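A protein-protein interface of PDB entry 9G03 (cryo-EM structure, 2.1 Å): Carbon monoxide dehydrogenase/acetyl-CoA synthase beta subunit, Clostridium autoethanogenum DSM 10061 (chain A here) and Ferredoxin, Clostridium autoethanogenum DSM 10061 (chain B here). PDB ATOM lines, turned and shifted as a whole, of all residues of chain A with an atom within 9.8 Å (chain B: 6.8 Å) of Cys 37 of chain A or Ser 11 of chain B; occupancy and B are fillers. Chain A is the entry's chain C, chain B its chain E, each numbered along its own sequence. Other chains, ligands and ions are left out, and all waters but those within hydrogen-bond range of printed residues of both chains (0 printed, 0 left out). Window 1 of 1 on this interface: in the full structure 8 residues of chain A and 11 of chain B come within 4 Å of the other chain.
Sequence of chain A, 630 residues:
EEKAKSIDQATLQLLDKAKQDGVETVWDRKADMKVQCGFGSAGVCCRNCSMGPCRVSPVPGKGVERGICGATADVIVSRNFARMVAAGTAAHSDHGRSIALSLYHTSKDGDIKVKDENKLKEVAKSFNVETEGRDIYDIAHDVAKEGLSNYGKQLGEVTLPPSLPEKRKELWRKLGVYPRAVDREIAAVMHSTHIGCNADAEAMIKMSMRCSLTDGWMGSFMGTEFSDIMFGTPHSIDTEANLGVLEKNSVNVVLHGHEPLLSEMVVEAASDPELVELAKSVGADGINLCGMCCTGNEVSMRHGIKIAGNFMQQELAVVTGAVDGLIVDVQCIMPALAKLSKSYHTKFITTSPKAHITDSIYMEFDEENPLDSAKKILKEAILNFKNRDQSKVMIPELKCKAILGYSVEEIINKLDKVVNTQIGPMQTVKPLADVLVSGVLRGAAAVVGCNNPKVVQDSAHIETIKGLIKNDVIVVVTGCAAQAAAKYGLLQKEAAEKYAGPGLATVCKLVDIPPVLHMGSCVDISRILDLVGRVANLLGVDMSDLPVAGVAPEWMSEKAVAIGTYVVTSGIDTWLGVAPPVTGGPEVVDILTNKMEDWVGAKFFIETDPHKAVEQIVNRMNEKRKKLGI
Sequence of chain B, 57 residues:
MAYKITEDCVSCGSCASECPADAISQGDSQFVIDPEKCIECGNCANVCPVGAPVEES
Gln 26 of chain B touches Met 33 of chain A (NE2 to O, 3.7 Å). CE of Lys 34 of chain A touches CB of Gln 26 of chain B, 3.2 Å away. OG of Ser 11 of chain B touches CG1 of Val 35 of chain A, at 3.2 Å. CG2 of Val 35 of chain A touches O of Gly 27 of chain B, at 3.6 Å. Val 35 of chain A touches Ser 29 of chain B. Val 35 of chain A touches Gln 30 of chain B (CG2 to N, 3.96 Å). O of Ser 11 of chain B touches CA of Cys 37 of chain A, at 3.4 Å. Val 10 of chain B touches Phe 39 of chain A (CG2 to CE2, 3.5 Å). Phe 39 of chain A touches Cys 12 of chain B (CE2 to CB, 3.7 Å).
The side-chain amide nitrogen (NE2) of Gln 26 of chain B sits at hydrogen-bond distance from the backbone carbonyl oxygen (O) of Val 35 of chain A (2.7 Å). N of Gly 38 of chain A lies within hydrogen-bond range of O of Val 10 of chain B, 2.9 Å away. NH1 of Arg 55 of chain A sits close to SG of Cys 12 of chain B, at 3.7 Å. The guanidinium group (NH2) of Arg 55 of chain A lies within hydrogen-bond range of the side-chain hydroxyl (OG) of Ser 14 of chain B (3.0 Å).
Printed residues of chain B that touch a printed residue of chain A: Val 10, Ser 11, Cys 12, Ser 14, Gln 26, Gly 27, Ser 29 and Gln 30. Hydrophobic or aromatic side chains of chain B within 4 Å of the printed part of chain A: Val 10. Of the 23 printed residues of chain A, 7 touch a printed residue of chain B. Printed residues of chain A that touch a printed residue of chain B: Met 33, Lys 34, Val 35, Cys 37, Gly 38, Phe 39 and Arg 55. Hydrophobic or aromatic side chains of chain A within 4 Å of the printed part of chain B: Val 35 and Phe 39. Among the printed residues, no Asp or Glu carboxylate lies within 4 Å of a Lys or Arg side-chain nitrogen of the other chain.
Of the printed residues of chain B, Cys 37 of chain A touches Ser 11. Of chain A, only Val 35 (3.2 Å) and Cys 37 (3.4 Å) come within 4 Å of Ser 11 of chain B. No residue of chain A comes within 4 Å of Cys 9 of chain B. Printed residues of chain A within 4 Å of Ser 29 of chain B: Val 35. Printed residues of chain A within 4 Å of Gln 26 of chain B: Met 33 (3.7 Å), Lys 34 (3.2 Å) and Val 35 (2.7 Å). Of the printed residues of chain A, Val 10 of chain B touches Gly 38 (2.9 Å) and Phe 39 (3.5 Å). Lys 454 of chain A touches none of the printed residues of chain B. The nearest printed residue of chain B that does not touch Cys 37 of chain A is Val 10 of chain B (4.01 Å). The nearest residue of chain A that does not touch Ser 11 of chain B is Gly 38 of chain A (4.1 Å).
The side-chain sulfur (SG) of Cys 37 of chain A sits close to the backbone NH (N) of Phe 39 of chain A. N of Gly 40 of chain A lies close to SG of Cys 37 of chain A (3.6 Å). The side-chain hydroxyl (OG) of Ser 41 of chain A is in hydrogen-bond range of the backbone carbonyl oxygen (O) of Cys 37 of chain A (2.8 Å). The backbone NH of Val 44 of chain A sits at hydrogen-bond distance from the backbone carbonyl oxygen of Phe 39 of chain A (3.0 Å). The side-chain sulfur of Cys 9 of chain B sits close to the backbone NH of Ser 11 of chain B (3.2 Å). OG of Ser 14 of chain B sits close to SG of Cys 12 of chain B, 3.3 Å away.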
ATOM      1  N   LYS A  30     -12.656 -14.375   8.980  1.00  0.00           N
ATOM      2  CA  LYS A  30     -11.419 -14.569   8.233  1.00  0.00           C
ATOM      3  C   LYS A  30     -10.398 -13.496   8.591  1.00  0.00           C
ATOM      4  O   LYS A  30      -9.224 -13.803   8.808  1.00  0.00           O
ATOM      5  CB  LYS A  30     -11.690 -14.569   6.724  1.00  0.00           C
ATOM      6  CG  LYS A  30     -10.428 -14.554   5.852  1.00  0.00           C
ATOM      7  CD  LYS A  30      -9.615 -15.829   6.030  1.00  0.00           C
ATOM      8  CE  LYS A  30      -8.506 -15.989   4.996  1.00  0.00           C
ATOM      9  NZ  LYS A  30      -7.517 -14.888   5.031  1.00  0.00           N
ATOM     10  N   MET A  33      -8.927 -14.244  11.986  1.00  0.00           N
ATOM     11  CA  MET A  33      -7.949 -15.319  11.990  1.00  0.00           C
ATOM     12  C   MET A  33      -6.557 -14.825  11.614  1.00  0.00           C
ATOM     13  O   MET A  33      -5.573 -15.503  11.916  1.00  0.00           O
ATOM     14  CB  MET A  33      -8.408 -16.427  11.041  1.00  0.00           C
ATOM     15  CG  MET A  33      -7.799 -17.774  11.327  1.00  0.00           C
ATOM     16  SD  MET A  33      -8.078 -18.387  13.012  1.00  0.00           S
ATOM     17  CE  MET A  33      -9.854 -18.606  13.036  1.00  0.00           C
ATOM     18  N   LYS A  34      -6.453 -13.683  10.934  1.00  0.00           N
ATOM     19  CA  LYS A  34      -5.170 -13.099  10.552  1.00  0.00           C
ATOM     20  C   LYS A  34      -4.288 -14.089   9.793  1.00  0.00           C
ATOM     21  O   LYS A  34      -4.792 -14.897   9.011  1.00  0.00           O
ATOM     22  CB  LYS A  34      -4.460 -12.558  11.801  1.00  0.00           C
ATOM     23  CG  LYS A  34      -5.245 -11.451  12.501  1.00  0.00           C
ATOM     24  CD  LYS A  34      -4.369 -10.551  13.345  1.00  0.00           C
ATOM     25  CE  LYS A  34      -4.005 -11.198  14.654  1.00  0.00           C
ATOM     26  NZ  LYS A  34      -5.116 -11.333  15.627  1.00  0.00           N
ATOM     27  N   VAL A  35      -2.975 -14.050  10.027  1.00  0.00           N
ATOM     28  CA  VAL A  35      -2.061 -14.939   9.320  1.00  0.00           C
ATOM     29  C   VAL A  35      -2.284 -16.360   9.814  1.00  0.00           C
ATOM     30  O   VAL A  35      -2.096 -16.657  10.997  1.00  0.00           O
ATOM     31  CB  VAL A  35      -0.601 -14.504   9.513  1.00  0.00           C
ATOM     32  CG1 VAL A  35       0.331 -15.428   8.745  1.00  0.00           C
ATOM     33  CG2 VAL A  35      -0.407 -13.073   9.054  1.00  0.00           C
ATOM     34  N   GLN A  36      -2.738 -17.228   8.927  1.00  0.00           N
ATOM     35  CA  GLN A  36      -3.020 -18.604   9.300  1.00  0.00           C
ATOM     36  C   GLN A  36      -1.724 -19.412   9.420  1.00  0.00           C
ATOM     37  O   GLN A  36      -0.706 -19.101   8.803  1.00  0.00           O
ATOM     38  CB  GLN A  36      -3.978 -19.236   8.303  1.00  0.00           C
ATOM     39  CG  GLN A  36      -5.369 -18.630   8.365  1.00  0.00           C
ATOM     40  CD  GLN A  36      -6.279 -19.188   7.300  1.00  0.00           C
ATOM     41  OE1 GLN A  36      -5.987 -19.083   6.116  1.00  0.00           O
ATOM     42  NE2 GLN A  36      -7.373 -19.805   7.713  1.00  0.00           N
ATOM     43  N   CYS A  37      -1.788 -20.483  10.208  1.00  0.00           N
ATOM     44  CA  CYS A  37      -0.586 -21.235  10.542  1.00  0.00           C
ATOM     45  C   CYS A  37       0.092 -21.772   9.286  1.00  0.00           C
ATOM     46  O   CYS A  37      -0.514 -22.497   8.497  1.00  0.00           O
ATOM     47  CB  CYS A  37      -0.939 -22.398  11.468  1.00  0.00           C
ATOM     48  SG  CYS A  37       0.458 -23.498  11.784  1.00  0.00           S
ATOM     49  N   GLY A  38       1.390 -21.487   9.166  1.00  0.00           N
ATOM     50  CA  GLY A  38       2.136 -21.924   7.996  1.00  0.00           C
ATOM     51  C   GLY A  38       2.255 -23.435   7.876  1.00  0.00           C
ATOM     52  O   GLY A  38       2.154 -23.984   6.777  1.00  0.00           O
ATOM     53  N   PHE A  39       2.443 -24.130   9.006  1.00  0.00           N
ATOM     54  CA  PHE A  39       2.567 -25.587   8.978  1.00  0.00           C
ATOM     55  C   PHE A  39       1.293 -26.237   8.461  1.00  0.00           C
ATOM     56  O   PHE A  39       1.338 -27.124   7.607  1.00  0.00           O
ATOM     57  CB  PHE A  39       2.895 -26.128  10.375  1.00  0.00           C
ATOM     58  CG  PHE A  39       4.203 -25.660  10.927  1.00  0.00           C
ATOM     59  CD1 PHE A  39       5.397 -26.196  10.473  1.00  0.00           C
ATOM     60  CD2 PHE A  39       4.243 -24.692  11.918  1.00  0.00           C
ATOM     61  CE1 PHE A  39       6.601 -25.769  10.989  1.00  0.00           C
ATOM     62  CE2 PHE A  39       5.449 -24.262  12.426  1.00  0.00           C
ATOM     63  CZ  PHE A  39       6.626 -24.804  11.964  1.00  0.00           C
ATOM     64  N   GLY A  40       0.143 -25.821   8.993  1.00  0.00           N
ATOM     65  CA  GLY A  40      -1.121 -26.360   8.524  1.00  0.00           C
ATOM     66  C   GLY A  40      -1.421 -25.973   7.087  1.00  0.00           C
ATOM     67  O   GLY A  40      -2.036 -26.739   6.343  1.00  0.00           O
ATOM     68  N   SER A  41      -1.039 -24.759   6.697  1.00  0.00           N
ATOM     69  CA  SER A  41      -1.266 -24.320   5.321  1.00  0.00           C
ATOM     70  C   SER A  41      -0.456 -25.152   4.333  1.00  0.00           C
ATOM     71  O   SER A  41      -0.924 -25.435   3.229  1.00  0.00           O
ATOM     72  CB  SER A  41      -0.927 -22.837   5.166  1.00  0.00           C
ATOM     73  OG  SER A  41      -1.702 -22.054   6.042  1.00  0.00           O
ATOM     74  N   ALA A  42       0.765 -25.541   4.705  1.00  0.00           N
ATOM     75  CA  ALA A  42       1.598 -26.379   3.851  1.00  0.00           C
ATOM     76  C   ALA A  42       1.312 -27.871   3.996  1.00  0.00           C
ATOM     77  O   ALA A  42       1.853 -28.660   3.219  1.00  0.00           O
ATOM     78  CB  ALA A  42       3.078 -26.118   4.132  1.00  0.00           C
ATOM     79  N   GLY A  43       0.516 -28.271   4.982  1.00  0.00           N
ATOM     80  CA  GLY A  43       0.188 -29.663   5.205  1.00  0.00           C
ATOM     81  C   GLY A  43       1.253 -30.478   5.907  1.00  0.00           C
ATOM     82  O   GLY A  43       1.175 -31.704   5.898  1.00  0.00           O
ATOM     83  N   VAL A  44       2.229 -29.833   6.546  1.00  0.00           N
ATOM     84  CA  VAL A  44       3.329 -30.517   7.223  1.00  0.00           C
ATOM     85  C   VAL A  44       3.076 -30.681   8.723  1.00  0.00           C
ATOM     86  O   VAL A  44       4.004 -30.989   9.470  1.00  0.00           O
ATOM     87  CB  VAL A  44       4.673 -29.824   6.953  1.00  0.00           C
ATOM     88  CG1 VAL A  44       5.132 -30.156   5.555  1.00  0.00           C
ATOM     89  CG2 VAL A  44       4.563 -28.316   7.137  1.00  0.00           C
ATOM     90  N   CYS A  45       1.864 -30.419   9.188  1.00  0.00           N
ATOM     91  CA  CYS A  45       1.494 -30.679  10.571  1.00  0.00           C
ATOM     92  C   CYS A  45       0.730 -31.990  10.629  1.00  0.00           C
ATOM     93  O   CYS A  45      -0.105 -32.267   9.767  1.00  0.00           O
ATOM     94  CB  CYS A  45       0.644 -29.562  11.176  1.00  0.00           C
ATOM     95  SG  CYS A  45       0.039 -29.941  12.859  1.00  0.00           S
ATOM     96  N   CYS A  46       1.022 -32.795  11.643  1.00  0.00           N
ATOM     97  CA  CYS A  46       0.348 -34.070  11.831  1.00  0.00           C
ATOM     98  C   CYS A  46      -0.191 -34.173  13.250  1.00  0.00           C
ATOM     99  O   CYS A  46       0.463 -33.760  14.207  1.00  0.00           O
ATOM    100  CB  CYS A  46       1.281 -35.244  11.550  1.00  0.00           C
ATOM    101  SG  CYS A  46       0.438 -36.831  11.639  1.00  0.00           S
ATOM    102  N   ARG A  47      -1.396 -34.712  13.372  1.00  0.00           N
ATOM    103  CA  ARG A  47      -1.991 -34.966  14.678  1.00  0.00           C
ATOM    104  C   ARG A  47      -2.628 -36.346  14.734  1.00  0.00           C
ATOM    105  O   ARG A  47      -3.565 -36.570  15.504  1.00  0.00           O
ATOM    106  CB  ARG A  47      -3.021 -33.892  15.033  1.00  0.00           C
ATOM    107  CG  ARG A  47      -2.445 -32.482  15.138  1.00  0.00           C
ATOM    108  CD  ARG A  47      -3.431 -31.524  15.805  1.00  0.00           C
ATOM    109  NE  ARG A  47      -4.708 -31.496  15.107  1.00  0.00           N
ATOM    110  CZ  ARG A  47      -5.068 -30.588  14.213  1.00  0.00           C
ATOM    111  NH1 ARG A  47      -4.279 -29.573  13.896  1.00  0.00           N
ATOM    112  NH2 ARG A  47      -6.257 -30.691  13.629  1.00  0.00           N
ATOM    113  N   CYS A  54       2.949 -33.194  15.700  1.00  0.00           N
ATOM    114  CA  CYS A  54       4.255 -33.086  15.063  1.00  0.00           C
ATOM    115  C   CYS A  54       4.144 -32.124  13.892  1.00  0.00           C
ATOM    116  O   CYS A  54       3.208 -32.211  13.089  1.00  0.00           O
ATOM    117  CB  CYS A  54       4.788 -34.441  14.564  1.00  0.00           C
ATOM    118  SG  CYS A  54       5.123 -35.715  15.811  1.00  0.00           S
ATOM    119  N   ARG A  55       5.101 -31.218  13.794  1.00  0.00           N
ATOM    120  CA  ARG A  55       5.238 -30.339  12.646  1.00  0.00           C
ATOM    121  C   ARG A  55       6.659 -30.456  12.131  1.00  0.00           C
ATOM    122  O   ARG A  55       7.618 -30.425  12.906  1.00  0.00           O
ATOM    123  CB  ARG A  55       4.880 -28.885  12.979  1.00  0.00           C
ATOM    124  CG  ARG A  55       5.433 -28.362  14.262  1.00  0.00           C
ATOM    125  CD  ARG A  55       4.756 -27.078  14.643  1.00  0.00           C
ATOM    126  NE  ARG A  55       5.283 -26.580  15.900  1.00  0.00           N
ATOM    127  CZ  ARG A  55       4.739 -25.624  16.631  1.00  0.00           C
ATOM    128  NH1 ARG A  55       3.642 -24.990  16.245  1.00  0.00           N
ATOM    129  NH2 ARG A  55       5.307 -25.297  17.784  1.00  0.00           N
ATOM    130  N   VAL A  56       6.775 -30.686  10.838  1.00  0.00           N
ATOM    131  CA  VAL A  56       8.060 -30.774  10.177  1.00  0.00           C
ATOM    132  C   VAL A  56       8.184 -29.581   9.239  1.00  0.00           C
ATOM    133  O   VAL A  56       7.200 -28.936   8.869  1.00  0.00           O
ATOM    134  CB  VAL A  56       8.227 -32.111   9.426  1.00  0.00           C
ATOM    135  CG1 VAL A  56       8.190 -33.284  10.417  1.00  0.00           C
ATOM    136  CG2 VAL A  56       7.157 -32.263   8.332  1.00  0.00           C
ATOM    137  N   PRO A  58       8.308 -27.251   6.178  1.00  0.00           N
ATOM    138  CA  PRO A  58       7.865 -27.257   4.777  1.00  0.00           C
ATOM    139  C   PRO A  58       8.995 -27.071   3.774  1.00  0.00           C
ATOM    140  O   PRO A  58       8.781 -27.313   2.586  1.00  0.00           O
ATOM    141  CB  PRO A  58       6.875 -26.087   4.724  1.00  0.00           C
ATOM    142  CG  PRO A  58       7.325 -25.176   5.780  1.00  0.00           C
ATOM    143  CD  PRO A  58       7.871 -26.034   6.883  1.00  0.00           C
ATOM    144  N   LYS A 454     -10.477 -16.548   0.893  1.00  0.00           N
ATOM    145  CA  LYS A 454      -9.166 -16.266   0.317  1.00  0.00           C
ATOM    146  C   LYS A 454      -9.252 -15.645  -1.077  1.00  0.00           C
ATOM    147  O   LYS A 454      -8.288 -15.014  -1.514  1.00  0.00           O
ATOM    148  CB  LYS A 454      -8.329 -17.546   0.246  1.00  0.00           C
ATOM    149  CG  LYS A 454      -7.956 -18.107   1.603  1.00  0.00           C
ATOM    150  CD  LYS A 454      -7.404 -19.513   1.508  1.00  0.00           C
ATOM    151  CE  LYS A 454      -7.030 -20.037   2.890  1.00  0.00           C
ATOM    152  NZ  LYS A 454      -6.463 -21.406   2.821  1.00  0.00           N
ATOM    153  N   PRO A 581      -3.431 -27.842   0.820  1.00  0.00           N
ATOM    154  CA  PRO A 581      -2.271 -27.900   1.733  1.00  0.00           C
ATOM    155  C   PRO A 581      -1.308 -29.041   1.423  1.00  0.00           C
ATOM    156  O   PRO A 581      -1.283 -30.051   2.128  1.00  0.00           O
ATOM    157  CB  PRO A 581      -2.925 -28.063   3.112  1.00  0.00           C
ATOM    158  CG  PRO A 581      -4.222 -28.728   2.833  1.00  0.00           C
ATOM    159  CD  PRO A 581      -4.685 -28.210   1.502  1.00  0.00           C
ATOM    160  N   THR A 583       1.933 -28.002  -0.375  1.00  0.00           N
ATOM    161  CA  THR A 583       3.197 -27.397  -0.779  1.00  0.00           C
ATOM    162  C   THR A 583       4.348 -27.836   0.114  1.00  0.00           C
ATOM    163  O   THR A 583       5.505 -27.718  -0.294  1.00  0.00           O
ATOM    164  CB  THR A 583       3.093 -25.864  -0.803  1.00  0.00           C
ATOM    165  OG1 THR A 583       2.757 -25.376   0.499  1.00  0.00           O
ATOM    166  CG2 THR A 583       2.035 -25.411  -1.809  1.00  0.00           C
ATOM    167  N   ASP B   8      11.293 -14.896   8.894  1.00  0.00           N
ATOM    168  CA  ASP B   8      11.329 -16.352   8.938  1.00  0.00           C
ATOM    169  C   ASP B   8      10.099 -16.924   9.636  1.00  0.00           C
ATOM    170  O   ASP B   8       9.823 -18.122   9.506  1.00  0.00           O
ATOM    171  CB  ASP B   8      12.611 -16.805   9.639  1.00  0.00           C
ATOM    172  CG  ASP B   8      12.685 -18.308   9.816  1.00  0.00           C
ATOM    173  OD1 ASP B   8      12.563 -19.034   8.809  1.00  0.00           O
ATOM    174  OD2 ASP B   8      12.878 -18.762  10.963  1.00  0.00           O
ATOM    175  N   CYS B   9       9.362 -16.091  10.366  1.00  0.00           N
ATOM    176  CA  CYS B   9       8.196 -16.533  11.122  1.00  0.00           C
ATOM    177  C   CYS B   9       7.115 -17.098  10.211  1.00  0.00           C
ATOM    178  O   CYS B   9       6.746 -16.483   9.209  1.00  0.00           O
ATOM    179  CB  CYS B   9       7.631 -15.360  11.925  1.00  0.00           C
ATOM    180  SG  CYS B   9       6.041 -15.683  12.717  1.00  0.00           S
ATOM    181  N   VAL B  10       6.624 -18.290  10.554  1.00  0.00           N
ATOM    182  CA  VAL B  10       5.528 -18.918   9.825  1.00  0.00           C
ATOM    183  C   VAL B  10       4.213 -18.800  10.583  1.00  0.00           C
ATOM    184  O   VAL B  10       3.230 -19.453  10.223  1.00  0.00           O
ATOM    185  CB  VAL B  10       5.833 -20.387   9.493  1.00  0.00           C
ATOM    186  CG1 VAL B  10       7.028 -20.476   8.571  1.00  0.00           C
ATOM    187  CG2 VAL B  10       6.067 -21.199  10.759  1.00  0.00           C
ATOM    188  N   SER B  11       4.186 -18.018  11.662  1.00  0.00           N
ATOM    189  CA  SER B  11       2.966 -17.746  12.410  1.00  0.00           C
ATOM    190  C   SER B  11       2.363 -19.018  13.008  1.00  0.00           C
ATOM    191  O   SER B  11       1.230 -19.399  12.713  1.00  0.00           O
ATOM    192  CB  SER B  11       1.959 -17.016  11.518  1.00  0.00           C
ATOM    193  OG  SER B  11       2.518 -15.804  11.054  1.00  0.00           O
ATOM    194  N   CYS B  12       3.138 -19.669  13.870  1.00  0.00           N
ATOM    195  CA  CYS B  12       2.647 -20.856  14.556  1.00  0.00           C
ATOM    196  C   CYS B  12       2.058 -20.531  15.929  1.00  0.00           C
ATOM    197  O   CYS B  12       1.446 -21.406  16.547  1.00  0.00           O
ATOM    198  CB  CYS B  12       3.770 -21.890  14.703  1.00  0.00           C
ATOM    199  SG  CYS B  12       4.987 -21.516  15.969  1.00  0.00           S
ATOM    200  N   GLY B  13       2.208 -19.295  16.401  1.00  0.00           N
ATOM    201  CA  GLY B  13       1.628 -18.824  17.643  1.00  0.00           C
ATOM    202  C   GLY B  13       2.281 -19.277  18.933  1.00  0.00           C
ATOM    203  O   GLY B  13       1.765 -18.948  20.009  1.00  0.00           O
ATOM    204  N   SER B  14       3.384 -20.018  18.878  1.00  0.00           N
ATOM    205  CA  SER B  14       3.980 -20.564  20.097  1.00  0.00           C
ATOM    206  C   SER B  14       4.589 -19.467  20.970  1.00  0.00           C
ATOM    207  O   SER B  14       4.353 -19.406  22.193  1.00  0.00           O
ATOM    208  CB  SER B  14       5.033 -21.600  19.730  1.00  0.00           C
ATOM    209  OG  SER B  14       4.450 -22.655  19.006  1.00  0.00           O
ATOM    210  N   GLN B  26       0.083 -11.040  17.314  1.00  0.00           N
ATOM    211  CA  GLN B  26      -0.103 -11.399  15.910  1.00  0.00           C
ATOM    212  C   GLN B  26      -0.366 -10.153  15.066  1.00  0.00           C
ATOM    213  O   GLN B  26      -1.170  -9.295  15.440  1.00  0.00           O
ATOM    214  CB  GLN B  26      -1.220 -12.426  15.758  1.00  0.00           C
ATOM    215  CG  GLN B  26      -1.303 -13.023  14.351  1.00  0.00           C
ATOM    216  CD  GLN B  26      -2.180 -14.265  14.281  1.00  0.00           C
ATOM    217  OE1 GLN B  26      -2.923 -14.566  15.213  1.00  0.00           O
ATOM    218  NE2 GLN B  26      -2.092 -14.994  13.172  1.00  0.00           N
ATOM    219  N   GLY B  27       0.324 -10.054  13.927  1.00  0.00           N
ATOM    220  CA  GLY B  27       0.179  -8.922  13.028  1.00  0.00           C
ATOM    221  C   GLY B  27      -0.235  -9.237  11.600  1.00  0.00           C
ATOM    222  O   GLY B  27      -0.825 -10.288  11.334  1.00  0.00           O
ATOM    223  N   SER B  29       1.523  -9.848   8.698  1.00  0.00           N
ATOM    224  CA  SER B  29       2.203 -10.910   7.970  1.00  0.00           C
ATOM    225  C   SER B  29       2.930 -11.882   8.881  1.00  0.00           C
ATOM    226  O   SER B  29       3.364 -12.939   8.411  1.00  0.00           O
ATOM    227  CB  SER B  29       3.205 -10.323   6.963  1.00  0.00           C
ATOM    228  OG  SER B  29       4.029  -9.342   7.565  1.00  0.00           O
ATOM    229  N   GLN B  30       3.080 -11.550  10.156  1.00  0.00           N
ATOM    230  CA  GLN B  30       3.830 -12.355  11.105  1.00  0.00           C
ATOM    231  C   GLN B  30       3.541 -11.796  12.488  1.00  0.00           C
ATOM    232  O   GLN B  30       3.002 -10.696  12.632  1.00  0.00           O
ATOM    233  CB  GLN B  30       5.327 -12.317  10.809  1.00  0.00           C
ATOM    234  CG  GLN B  30       5.941 -10.951  11.047  1.00  0.00           C
ATOM    235  CD  GLN B  30       7.410 -10.914  10.730  1.00  0.00           C
ATOM    236  OE1 GLN B  30       7.853 -11.496   9.744  1.00  0.00           O
ATOM    237  NE2 GLN B  30       8.179 -10.233  11.566  1.00  0.00           N
ATOM    238  N   PHE B  31       3.888 -12.573  13.504  1.00  0.00           N
ATOM    239  CA  PHE B  31       3.844 -12.059  14.863  1.00  0.00           C
ATOM    240  C   PHE B  31       4.918 -10.986  15.020  1.00  0.00           C
ATOM    241  O   PHE B  31       5.903 -10.958  14.283  1.00  0.00           O
ATOM    242  CB  PHE B  31       4.027 -13.198  15.864  1.00  0.00           C
ATOM    243  CG  PHE B  31       2.808 -14.069  16.004  1.00  0.00           C
ATOM    244  CD1 PHE B  31       2.447 -14.949  14.999  1.00  0.00           C
ATOM    245  CD2 PHE B  31       2.017 -13.994  17.135  1.00  0.00           C
ATOM    246  CE1 PHE B  31       1.323 -15.742  15.123  1.00  0.00           C
ATOM    247  CE2 PHE B  31       0.895 -14.786  17.264  1.00  0.00           C
ATOM    248  CZ  PHE B  31       0.547 -15.661  16.257  1.00  0.00           C
ATOM    249  N   VAL B  50      11.170 -22.701  13.930  1.00  0.00           N
ATOM    250  CA  VAL B  50      11.977 -22.177  12.833  1.00  0.00           C
ATOM    251  C   VAL B  50      13.038 -21.207  13.318  1.00  0.00           C
ATOM    252  O   VAL B  50      13.845 -20.738  12.501  1.00  0.00           O
ATOM    253  CB  VAL B  50      11.106 -21.508  11.745  1.00  0.00           C
ATOM    254  CG1 VAL B  50      10.134 -22.515  11.138  1.00  0.00           C
ATOM    255  CG2 VAL B  50      10.366 -20.306  12.308  1.00  0.00           C
